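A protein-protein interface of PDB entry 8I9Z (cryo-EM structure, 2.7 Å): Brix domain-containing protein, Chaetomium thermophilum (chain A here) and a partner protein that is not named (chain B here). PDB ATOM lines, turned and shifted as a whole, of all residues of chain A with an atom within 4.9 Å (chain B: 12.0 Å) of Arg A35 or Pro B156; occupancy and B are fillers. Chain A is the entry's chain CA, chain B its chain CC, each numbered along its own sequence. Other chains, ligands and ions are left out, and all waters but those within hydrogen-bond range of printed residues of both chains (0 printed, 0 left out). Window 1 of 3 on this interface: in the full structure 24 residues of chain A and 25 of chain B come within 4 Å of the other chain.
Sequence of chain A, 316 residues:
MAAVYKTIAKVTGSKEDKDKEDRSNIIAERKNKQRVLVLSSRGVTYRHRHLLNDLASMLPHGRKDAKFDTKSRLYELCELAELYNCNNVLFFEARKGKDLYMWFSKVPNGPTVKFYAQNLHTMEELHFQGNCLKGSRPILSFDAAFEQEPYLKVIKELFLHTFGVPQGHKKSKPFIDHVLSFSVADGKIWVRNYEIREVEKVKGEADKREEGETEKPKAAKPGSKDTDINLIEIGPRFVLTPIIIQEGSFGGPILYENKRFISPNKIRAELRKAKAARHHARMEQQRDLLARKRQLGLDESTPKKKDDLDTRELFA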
ATOM      1  N   SER A  24     -26.793 -18.600 -27.421  1.00  0.00           N
ATOM      2  CA  SER A  24     -27.710 -19.379 -26.604  1.00  0.00           C
ATOM      3  C   SER A  24     -27.022 -20.487 -25.825  1.00  0.00           C
ATOM      4  O   SER A  24     -27.681 -21.136 -25.007  1.00  0.00           O
ATOM      5  CB  SER A  24     -28.801 -19.994 -27.479  1.00  0.00           C
ATOM      6  OG  SER A  24     -28.236 -20.798 -28.496  1.00  0.00           O
ATOM      7  N   LYS A  33     -34.404 -23.078 -25.947  1.00  0.00           N
ATOM      8  CA  LYS A  33     -33.711 -22.051 -25.176  1.00  0.00           C
ATOM      9  C   LYS A  33     -34.484 -21.774 -23.895  1.00  0.00           C
ATOM     10  O   LYS A  33     -35.552 -21.157 -23.928  1.00  0.00           O
ATOM     11  CB  LYS A  33     -33.556 -20.783 -26.007  1.00  0.00           C
ATOM     12  CG  LYS A  33     -32.604 -20.918 -27.173  1.00  0.00           C
ATOM     13  CD  LYS A  33     -32.406 -19.590 -27.876  1.00  0.00           C
ATOM     14  CE  LYS A  33     -33.681 -19.119 -28.528  1.00  0.00           C
ATOM     15  NZ  LYS A  33     -33.466 -17.867 -29.298  1.00  0.00           N
ATOM     16  N   GLN A  34     -33.960 -22.243 -22.761  1.00  0.00           N
ATOM     17  CA  GLN A  34     -34.579 -22.005 -21.462  1.00  0.00           C
ATOM     18  C   GLN A  34     -33.516 -21.542 -20.481  1.00  0.00           C
ATOM     19  O   GLN A  34     -32.457 -22.161 -20.374  1.00  0.00           O
ATOM     20  CB  GLN A  34     -35.283 -23.256 -20.921  1.00  0.00           C
ATOM     21  CG  GLN A  34     -36.143 -24.001 -21.918  1.00  0.00           C
ATOM     22  CD  GLN A  34     -37.600 -23.615 -21.837  1.00  0.00           C
ATOM     23  OE1 GLN A  34     -37.940 -22.528 -21.378  1.00  0.00           O
ATOM     24  NE2 GLN A  34     -38.472 -24.504 -22.289  1.00  0.00           N
ATOM     25  N   ARG A  35     -33.801 -20.453 -19.771  1.00  0.00           N
ATOM     26  CA  ARG A  35     -32.973 -19.972 -18.674  1.00  0.00           C
ATOM     27  C   ARG A  35     -33.837 -19.809 -17.432  1.00  0.00           C
ATOM     28  O   ARG A  35     -34.908 -19.200 -17.490  1.00  0.00           O
ATOM     29  CB  ARG A  35     -32.304 -18.639 -19.013  1.00  0.00           C
ATOM     30  CG  ARG A  35     -31.359 -18.692 -20.182  1.00  0.00           C
ATOM     31  CD  ARG A  35     -29.963 -18.328 -19.746  1.00  0.00           C
ATOM     32  NE  ARG A  35     -29.759 -16.893 -19.608  1.00  0.00           N
ATOM     33  CZ  ARG A  35     -28.905 -16.342 -18.758  1.00  0.00           C
ATOM     34  NH1 ARG A  35     -28.181 -17.077 -17.934  1.00  0.00           N
ATOM     35  NH2 ARG A  35     -28.772 -15.020 -18.736  1.00  0.00           N
ATOM     36  N   VAL A  36     -33.371 -20.343 -16.308  1.00  0.00           N
ATOM     37  CA  VAL A  36     -34.118 -20.321 -15.057  1.00  0.00           C
ATOM     38  C   VAL A  36     -33.391 -19.412 -14.079  1.00  0.00           C
ATOM     39  O   VAL A  36     -32.176 -19.531 -13.903  1.00  0.00           O
ATOM     40  CB  VAL A  36     -34.285 -21.734 -14.468  1.00  0.00           C
ATOM     41  CG1 VAL A  36     -35.035 -21.684 -13.154  1.00  0.00           C
ATOM     42  CG2 VAL A  36     -35.008 -22.633 -15.446  1.00  0.00           C
ATOM     43  N   LEU A  37     -34.126 -18.496 -13.453  1.00  0.00           N
ATOM     44  CA  LEU A  37     -33.583 -17.651 -12.396  1.00  0.00           C
ATOM     45  C   LEU A  37     -34.015 -18.226 -11.051  1.00  0.00           C
ATOM     46  O   LEU A  37     -35.207 -18.239 -10.728  1.00  0.00           O
ATOM     47  CB  LEU A  37     -34.050 -16.207 -12.553  1.00  0.00           C
ATOM     48  CG  LEU A  37     -33.727 -15.292 -11.377  1.00  0.00           C
ATOM     49  CD1 LEU A  37     -32.286 -14.848 -11.443  1.00  0.00           C
ATOM     50  CD2 LEU A  37     -34.650 -14.095 -11.373  1.00  0.00           C
ATOM     51  N   HIS A  61     -28.502 -24.280 -16.638  1.00  0.00           N
ATOM     52  CA  HIS A  61     -29.062 -23.054 -17.174  1.00  0.00           C
ATOM     53  C   HIS A  61     -29.671 -22.180 -16.093  1.00  0.00           C
ATOM     54  O   HIS A  61     -30.519 -21.333 -16.394  1.00  0.00           O
ATOM     55  CB  HIS A  61     -30.105 -23.387 -18.239  1.00  0.00           C
ATOM     56  CG  HIS A  61     -31.195 -24.286 -17.750  1.00  0.00           C
ATOM     57  ND1 HIS A  61     -31.026 -25.641 -17.578  1.00  0.00           N
ATOM     58  CD2 HIS A  61     -32.476 -24.022 -17.406  1.00  0.00           C
ATOM     59  CE1 HIS A  61     -32.151 -26.171 -17.136  1.00  0.00           C
ATOM     60  NE2 HIS A  61     -33.048 -25.210 -17.026  1.00  0.00           N
ATOM     61  N   TYR A  84     -31.546 -10.496 -16.091  1.00  0.00           N
ATOM     62  CA  TYR A  84     -30.658 -11.646 -16.181  1.00  0.00           C
ATOM     63  C   TYR A  84     -30.976 -12.519 -17.381  1.00  0.00           C
ATOM     64  O   TYR A  84     -30.363 -13.580 -17.533  1.00  0.00           O
ATOM     65  CB  TYR A  84     -30.755 -12.469 -14.899  1.00  0.00           C
ATOM     66  CG  TYR A  84     -29.881 -11.956 -13.783  1.00  0.00           C
ATOM     67  CD1 TYR A  84     -28.574 -11.574 -14.015  1.00  0.00           C
ATOM     68  CD2 TYR A  84     -30.384 -11.822 -12.500  1.00  0.00           C
ATOM     69  CE1 TYR A  84     -27.782 -11.104 -12.992  1.00  0.00           C
ATOM     70  CE2 TYR A  84     -29.603 -11.345 -11.474  1.00  0.00           C
ATOM     71  CZ  TYR A  84     -28.301 -10.985 -11.726  1.00  0.00           C
ATOM     72  OH  TYR A  84     -27.516 -10.510 -10.701  1.00  0.00           O
ATOM     73  N   ASN A  85     -31.952 -12.102 -18.195  1.00  0.00           N
ATOM     74  CA  ASN A  85     -32.292 -12.701 -19.488  1.00  0.00           C
ATOM     75  C   ASN A  85     -32.817 -14.129 -19.314  1.00  0.00           C
ATOM     76  O   ASN A  85     -32.388 -15.059 -19.994  1.00  0.00           O
ATOM     77  CB  ASN A  85     -31.096 -12.654 -20.442  1.00  0.00           C
ATOM     78  CG  ASN A  85     -31.503 -12.440 -21.870  1.00  0.00           C
ATOM     79  OD1 ASN A  85     -32.679 -12.270 -22.169  1.00  0.00           O
ATOM     80  ND2 ASN A  85     -30.529 -12.433 -22.769  1.00  0.00           N
ATOM     81  N   CYS A  86     -33.763 -14.290 -18.390  1.00  0.00           N
ATOM     82  CA  CYS A  86     -34.298 -15.589 -18.008  1.00  0.00           C
ATOM     83  C   CYS A  86     -35.797 -15.631 -18.258  1.00  0.00           C
ATOM     84  O   CYS A  86     -36.514 -14.683 -17.928  1.00  0.00           O
ATOM     85  CB  CYS A  86     -34.026 -15.886 -16.530  1.00  0.00           C
ATOM     86  SG  CYS A  86     -32.290 -15.925 -16.070  1.00  0.00           S
ATOM     87  N   ASN A  87     -36.272 -16.740 -18.823  1.00  0.00           N
ATOM     88  CA  ASN A  87     -37.696 -16.923 -19.059  1.00  0.00           C
ATOM     89  C   ASN A  87     -38.369 -17.813 -18.025  1.00  0.00           C
ATOM     90  O   ASN A  87     -39.540 -18.159 -18.201  1.00  0.00           O
ATOM     91  CB  ASN A  87     -37.939 -17.483 -20.467  1.00  0.00           C
ATOM     92  CG  ASN A  87     -37.259 -18.812 -20.701  1.00  0.00           C
ATOM     93  OD1 ASN A  87     -36.407 -19.235 -19.928  1.00  0.00           O
ATOM     94  ND2 ASN A  87     -37.638 -19.480 -21.777  1.00  0.00           N
ATOM     95  N   ASN A  88     -37.672 -18.182 -16.954  1.00  0.00           N
ATOM     96  CA  ASN A  88     -38.265 -18.923 -15.851  1.00  0.00           C
ATOM     97  C   ASN A  88     -37.773 -18.350 -14.533  1.00  0.00           C
ATOM     98  O   ASN A  88     -36.604 -17.979 -14.410  1.00  0.00           O
ATOM     99  CB  ASN A  88     -37.919 -20.411 -15.913  1.00  0.00           C
ATOM    100  CG  ASN A  88     -38.185 -21.014 -17.265  1.00  0.00           C
ATOM    101  OD1 ASN A  88     -39.331 -21.197 -17.647  1.00  0.00           O
ATOM    102  ND2 ASN A  88     -37.128 -21.323 -18.004  1.00  0.00           N
ATOM    103  N   ASP B 152     -43.675  -8.567 -24.547  1.00  0.00           N
ATOM    104  CA  ASP B 152     -42.727  -9.186 -25.461  1.00  0.00           C
ATOM    105  C   ASP B 152     -41.995 -10.323 -24.766  1.00  0.00           C
ATOM    106  O   ASP B 152     -41.493 -10.161 -23.650  1.00  0.00           O
ATOM    107  CB  ASP B 152     -41.727  -8.151 -25.967  1.00  0.00           C
ATOM    108  CG  ASP B 152     -42.362  -6.804 -26.217  1.00  0.00           C
ATOM    109  OD1 ASP B 152     -42.794  -6.159 -25.240  1.00  0.00           O
ATOM    110  OD2 ASP B 152     -42.434  -6.389 -27.393  1.00  0.00           O
ATOM    111  N   GLU B 153     -41.935 -11.475 -25.423  1.00  0.00           N
ATOM    112  CA  GLU B 153     -41.296 -12.637 -24.830  1.00  0.00           C
ATOM    113  C   GLU B 153     -39.786 -12.448 -24.758  1.00  0.00           C
ATOM    114  O   GLU B 153     -39.164 -11.865 -25.650  1.00  0.00           O
ATOM    115  CB  GLU B 153     -41.631 -13.892 -25.631  1.00  0.00           C
ATOM    116  CG  GLU B 153     -43.057 -14.374 -25.444  1.00  0.00           C
ATOM    117  CD  GLU B 153     -43.165 -15.887 -25.441  1.00  0.00           C
ATOM    118  OE1 GLU B 153     -42.161 -16.556 -25.765  1.00  0.00           O
ATOM    119  OE2 GLU B 153     -44.253 -16.407 -25.118  1.00  0.00           O
ATOM    120  N   ILE B 154     -39.201 -12.944 -23.677  1.00  0.00           N
ATOM    121  CA  ILE B 154     -37.765 -12.837 -23.459  1.00  0.00           C
ATOM    122  C   ILE B 154     -37.044 -13.834 -24.356  1.00  0.00           C
ATOM    123  O   ILE B 154     -37.436 -15.001 -24.455  1.00  0.00           O
ATOM    124  CB  ILE B 154     -37.433 -13.074 -21.975  1.00  0.00           C
ATOM    125  CG1 ILE B 154     -38.125 -12.029 -21.106  1.00  0.00           C
ATOM    126  CG2 ILE B 154     -35.937 -13.030 -21.735  1.00  0.00           C
ATOM    127  CD1 ILE B 154     -37.863 -12.202 -19.637  1.00  0.00           C
ATOM    128  N   ASP B 155     -35.999 -13.368 -25.034  1.00  0.00           N
ATOM    129  CA  ASP B 155     -35.107 -14.261 -25.759  1.00  0.00           C
ATOM    130  C   ASP B 155     -34.049 -14.784 -24.797  1.00  0.00           C
ATOM    131  O   ASP B 155     -33.167 -14.028 -24.374  1.00  0.00           O
ATOM    132  CB  ASP B 155     -34.448 -13.537 -26.932  1.00  0.00           C
ATOM    133  CG  ASP B 155     -33.705 -14.476 -27.853  1.00  0.00           C
ATOM    134  OD1 ASP B 155     -33.879 -15.705 -27.727  1.00  0.00           O
ATOM    135  OD2 ASP B 155     -32.938 -13.982 -28.704  1.00  0.00           O
ATOM    136  N   PRO B 156     -34.085 -16.061 -24.442  1.00  0.00           N
ATOM    137  CA  PRO B 156     -33.152 -16.565 -23.431  1.00  0.00           C
ATOM    138  C   PRO B 156     -31.772 -16.824 -24.004  1.00  0.00           C
ATOM    139  O   PRO B 156     -31.406 -17.970 -24.281  1.00  0.00           O
ATOM    140  CB  PRO B 156     -33.817 -17.863 -22.953  1.00  0.00           C
ATOM    141  CG  PRO B 156     -35.154 -17.920 -23.651  1.00  0.00           C
ATOM    142  CD  PRO B 156     -35.007 -17.112 -24.884  1.00  0.00           C
ATOM    143  N   VAL B 157     -30.998 -15.762 -24.180  1.00  0.00           N
ATOM    144  CA  VAL B 157     -29.649 -15.861 -24.713  1.00  0.00           C
ATOM    145  C   VAL B 157     -28.686 -15.255 -23.705  1.00  0.00           C
ATOM    146  O   VAL B 157     -29.070 -14.446 -22.856  1.00  0.00           O
ATOM    147  CB  VAL B 157     -29.522 -15.162 -26.082  1.00  0.00           C
ATOM    148  CG1 VAL B 157     -30.288 -15.934 -27.140  1.00  0.00           C
ATOM    149  CG2 VAL B 157     -30.017 -13.733 -25.995  1.00  0.00           C
ATOM    150  N   TYR B 158     -27.428 -15.658 -23.799  1.00  0.00           N
ATOM    151  CA  TYR B 158     -26.412 -15.159 -22.888  1.00  0.00           C
ATOM    152  C   TYR B 158     -25.814 -13.873 -23.440  1.00  0.00           C
ATOM    153  O   TYR B 158     -25.397 -13.819 -24.600  1.00  0.00           O
ATOM    154  CB  TYR B 158     -25.319 -16.205 -22.671  1.00  0.00           C
ATOM    155  CG  TYR B 158     -25.730 -17.358 -21.782  1.00  0.00           C
ATOM    156  CD1 TYR B 158     -26.658 -18.302 -22.206  1.00  0.00           C
ATOM    157  CD2 TYR B 158     -25.213 -17.481 -20.503  1.00  0.00           C
ATOM    158  CE1 TYR B 158     -27.032 -19.345 -21.395  1.00  0.00           C
ATOM    159  CE2 TYR B 158     -25.588 -18.518 -19.681  1.00  0.00           C
ATOM    160  CZ  TYR B 158     -26.498 -19.447 -20.131  1.00  0.00           C
ATOM    161  OH  TYR B 158     -26.874 -20.484 -19.314  1.00  0.00           O
ATOM    162  N   ASP B 159     -25.775 -12.838 -22.611  1.00  0.00           N
ATOM    163  CA  ASP B 159     -25.244 -11.545 -23.005  1.00  0.00           C
ATOM    164  C   ASP B 159     -23.721 -11.540 -22.943  1.00  0.00           C
ATOM    165  O   ASP B 159     -23.088 -12.458 -22.420  1.00  0.00           O
ATOM    166  CB  ASP B 159     -25.816 -10.440 -22.123  1.00  0.00           C
ATOM    167  CG  ASP B 159     -27.153  -9.943 -22.614  1.00  0.00           C
ATOM    168  OD1 ASP B 159     -27.636 -10.460 -23.642  1.00  0.00           O
ATOM    169  OD2 ASP B 159     -27.722  -9.035 -21.976  1.00  0.00           O
ATOM    170  N   SER B 160     -23.137 -10.466 -23.480  1.00  0.00           N
ATOM    171  CA  SER B 160     -21.687 -10.377 -23.624  1.00  0.00           C
ATOM    172  C   SER B 160     -20.980 -10.280 -22.278  1.00  0.00           C
ATOM    173  O   SER B 160     -19.798 -10.619 -22.172  1.00  0.00           O
ATOM    174  CB  SER B 160     -21.336  -9.170 -24.497  1.00  0.00           C
ATOM    175  OG  SER B 160     -19.954  -8.882 -24.443  1.00  0.00           O
ATOM    176  N   ASP B 161     -21.679  -9.819 -21.248  1.00  0.00           N
ATOM    177  CA  ASP B 161     -21.108  -9.608 -19.926  1.00  0.00           C
ATOM    178  C   ASP B 161     -21.437 -10.726 -18.951  1.00  0.00           C
ATOM    179  O   ASP B 161     -21.089 -10.620 -17.772  1.00  0.00           O
ATOM    180  CB  ASP B 161     -21.604  -8.275 -19.362  1.00  0.00           C
ATOM    181  CG  ASP B 161     -23.097  -8.071 -19.573  1.00  0.00           C
ATOM    182  OD1 ASP B 161     -23.892  -8.937 -19.155  1.00  0.00           O
ATOM    183  OD2 ASP B 161     -23.480  -7.057 -20.188  1.00  0.00           O
ATOM    184  N   ASP B 162     -22.104 -11.780 -19.409  1.00  0.00           N
ATOM    185  CA  ASP B 162     -22.564 -12.831 -18.520  1.00  0.00           C
ATOM    186  C   ASP B 162     -21.391 -13.646 -17.992  1.00  0.00           C
ATOM    187  O   ASP B 162     -20.323 -13.714 -18.607  1.00  0.00           O
ATOM    188  CB  ASP B 162     -23.550 -13.742 -19.247  1.00  0.00           C
ATOM    189  CG  ASP B 162     -24.550 -14.383 -18.314  1.00  0.00           C
ATOM    190  OD1 ASP B 162     -24.128 -15.025 -17.329  1.00  0.00           O
ATOM    191  OD2 ASP B 162     -25.765 -14.246 -18.562  1.00  0.00           O
ATOM    192  N   THR B 163     -21.597 -14.249 -16.821  1.00  0.00           N
ATOM    193  CA  THR B 163     -20.574 -15.107 -16.234  1.00  0.00           C
ATOM    194  C   THR B 163     -20.336 -16.344 -17.090  1.00  0.00           C
ATOM    195  O   THR B 163     -19.194 -16.783 -17.261  1.00  0.00           O
ATOM    196  CB  THR B 163     -20.980 -15.507 -14.818  1.00  0.00           C
ATOM    197  OG1 THR B 163     -21.470 -14.357 -14.115  1.00  0.00           O
ATOM    198  CG2 THR B 163     -19.796 -16.084 -14.069  1.00  0.00           C
ATOM    199  N   ASP B 164     -21.405 -16.914 -17.645  1.00  0.00           N
ATOM    200  CA  ASP B 164     -21.329 -18.108 -18.474  1.00  0.00           C
ATOM    201  C   ASP B 164     -21.404 -17.784 -19.961  1.00  0.00           C
ATOM    202  O   ASP B 164     -21.971 -18.559 -20.737  1.00  0.00           O
ATOM    203  CB  ASP B 164     -22.436 -19.086 -18.086  1.00  0.00           C
ATOM    204  CG  ASP B 164     -22.737 -19.063 -16.604  1.00  0.00           C
ATOM    205  OD1 ASP B 164     -23.826 -18.587 -16.223  1.00  0.00           O
ATOM    206  OD2 ASP B 164     -21.882 -19.521 -15.815  1.00  0.00           O
ATOM    207  N   TYR B 165     -20.856 -16.640 -20.371  1.00  0.00           N
ATOM    208  CA  TYR B 165     -20.868 -16.275 -21.782  1.00  0.00           C
ATOM    209  C   TYR B 165     -19.931 -17.162 -22.586  1.00  0.00           C
ATOM    210  O   TYR B 165     -20.265 -17.575 -23.701  1.00  0.00           O
ATOM    211  CB  TYR B 165     -20.495 -14.804 -21.938  1.00  0.00           C
ATOM    212  CG  TYR B 165     -20.389 -14.325 -23.364  1.00  0.00           C
ATOM    213  CD1 TYR B 165     -21.460 -14.441 -24.235  1.00  0.00           C
ATOM    214  CD2 TYR B 165     -19.228 -13.730 -23.830  1.00  0.00           C
ATOM    215  CE1 TYR B 165     -21.373 -13.991 -25.534  1.00  0.00           C
ATOM    216  CE2 TYR B 165     -19.131 -13.281 -25.129  1.00  0.00           C
ATOM    217  CZ  TYR B 165     -20.207 -13.415 -25.975  1.00  0.00           C
ATOM    218  OH  TYR B 165     -20.117 -12.969 -27.272  1.00  0.00           O
ATOM    219  N   ASN B 166     -18.762 -17.472 -22.037  1.00  0.00           N
ATOM    220  CA  ASN B 166     -17.822 -18.404 -22.642  1.00  0.00           C
ATOM    221  C   ASN B 166     -17.760 -19.653 -21.778  1.00  0.00           C
ATOM    222  O   ASN B 166     -17.416 -19.576 -20.594  1.00  0.00           O
ATOM    223  CB  ASN B 166     -16.435 -17.781 -22.777  1.00  0.00           C
ATOM    224  CG  ASN B 166     -16.414 -16.623 -23.739  1.00  0.00           C
ATOM    225  OD1 ASN B 166     -17.384 -16.374 -24.449  1.00  0.00           O
ATOM    226  ND2 ASN B 166     -15.302 -15.900 -23.769  1.00  0.00           N
ATOM    227  N   VAL B 167     -18.087 -20.794 -22.364  1.00  0.00           N
ATOM    228  CA  VAL B 167     -18.096 -22.077 -21.669  1.00  0.00           C
ATOM    229  C   VAL B 167     -16.959 -22.922 -22.224  1.00  0.00           C
ATOM    230  O   VAL B 167     -16.838 -23.046 -23.448  1.00  0.00           O
ATOM    231  CB  VAL B 167     -19.440 -22.807 -21.830  1.00  0.00           C
ATOM    232  CG1 VAL B 167     -19.444 -24.086 -21.020  1.00  0.00           C
ATOM    233  CG2 VAL B 167     -20.575 -21.910 -21.395  1.00  0.00           C
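Printed residues of chain B that touch a printed residue of chain A: Ile B154, Asp B155, Pro B156, Val B157, Tyr B158, Asp B159 and Asp B162.
The backbone carbonyl oxygen (O) of Asn A85 is in hydrogen-bond range of the guanidinium group (NE) of Arg A35 (3.2 Å). The backbone carbonyl oxygen of Arg A35 lies close to the side-chain amide oxygen of Asn A87, at 2.9 Å. The backbone NH (N) of Asp B164 lies close to the side-chain carboxylate (OD1) of Asp B162, at 3.3 Å. The side-chain amide oxygen of Gln A34 is in hydrogen-bond range of the side-chain amide nitrogen of Asn A87, at 3.1 Å. OD1 of Asn A87 lies within hydrogen-bond range of ND2 of Asn A88. The backbone carbonyl oxygen of Lys A33 sits at hydrogen-bond distance from the side-chain amide nitrogen of Asn A87, 3.4 Å away.
NH2 of Arg A35 lies within salt-bridge range of OD2 of Asp B162 (3.1 Å). NZ of Lys A33 is in salt-bridge range of OD1 of Asp B155 (2.7 Å). The backbone carbonyl oxygen (O) of Asp B155 sits close to the side-chain amide oxygen (OD1) of Asn A85, 2.9 Å away. The side-chain amide nitrogen of Asn A85 lies within hydrogen-bond range of the backbone carbonyl oxygen of Val B157 (2.5 Å).
Lys A33 touches Pro B156. Arg A35 touches Pro B156. CE2 of Tyr B158 touches NH1 of Arg A35 (3.4 Å). Tyr B158 touches His A61 (OH to CA, 3.996 Å). Ile B154 touches Asn A85. Asn A85 touches Pro B156 (O to CA, 3.8 Å). Asn A85 touches Asp B159 (ND2 to OD1, 3.6 Å). Ile B154 touches Cys A86 (CD1 to O, 3.3 Å). CG of Pro B156 touches ND2 of Asn A87, at 3.5 Å.
No residue of chain B comes within 4 Å of Ser A24. Of chain B, only Asp B155 and Pro B156 come within 4 Å of Lys A33. No residue of chain B comes within 4 Å of Gln A34. Printed residues of chain B within 4 Å of Arg A35: Pro B156 (3.8 Å), Tyr B158 (3.4 Å) and Asp B162 (3.1 Å). Cys A86 touches just one residue of chain B: Ile B154. Of chain B, only Pro B156 (3.5 Å) comes within 4 Å of Asn A87. No residue of chain B comes within 4 Å of Asn A88. Of the printed residues of chain A, Ile B154 touches Asn A85 (3.4 Å) and Cys A86 (3.3 Å). Of the printed residues of chain A, Asp B155 touches Lys A33 (2.7 Å) and Asn A85 (2.9 Å). Of chain A, only Lys A33 (3.3 Å), Arg A35 (3.8 Å), Asn A85 (3.8 Å) and Asn A87 (3.5 Å) come within 4 Å of Pro B156. Printed residues of chain A within 4 Å of Val B157: Asn A85 (2.5 Å). The nearest residue of chain B that does not touch Arg A35 is Val B157 (4.1 Å). The nearest residue of chain A that does not touch Pro B156 is Gln A34 (4.4 Å).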
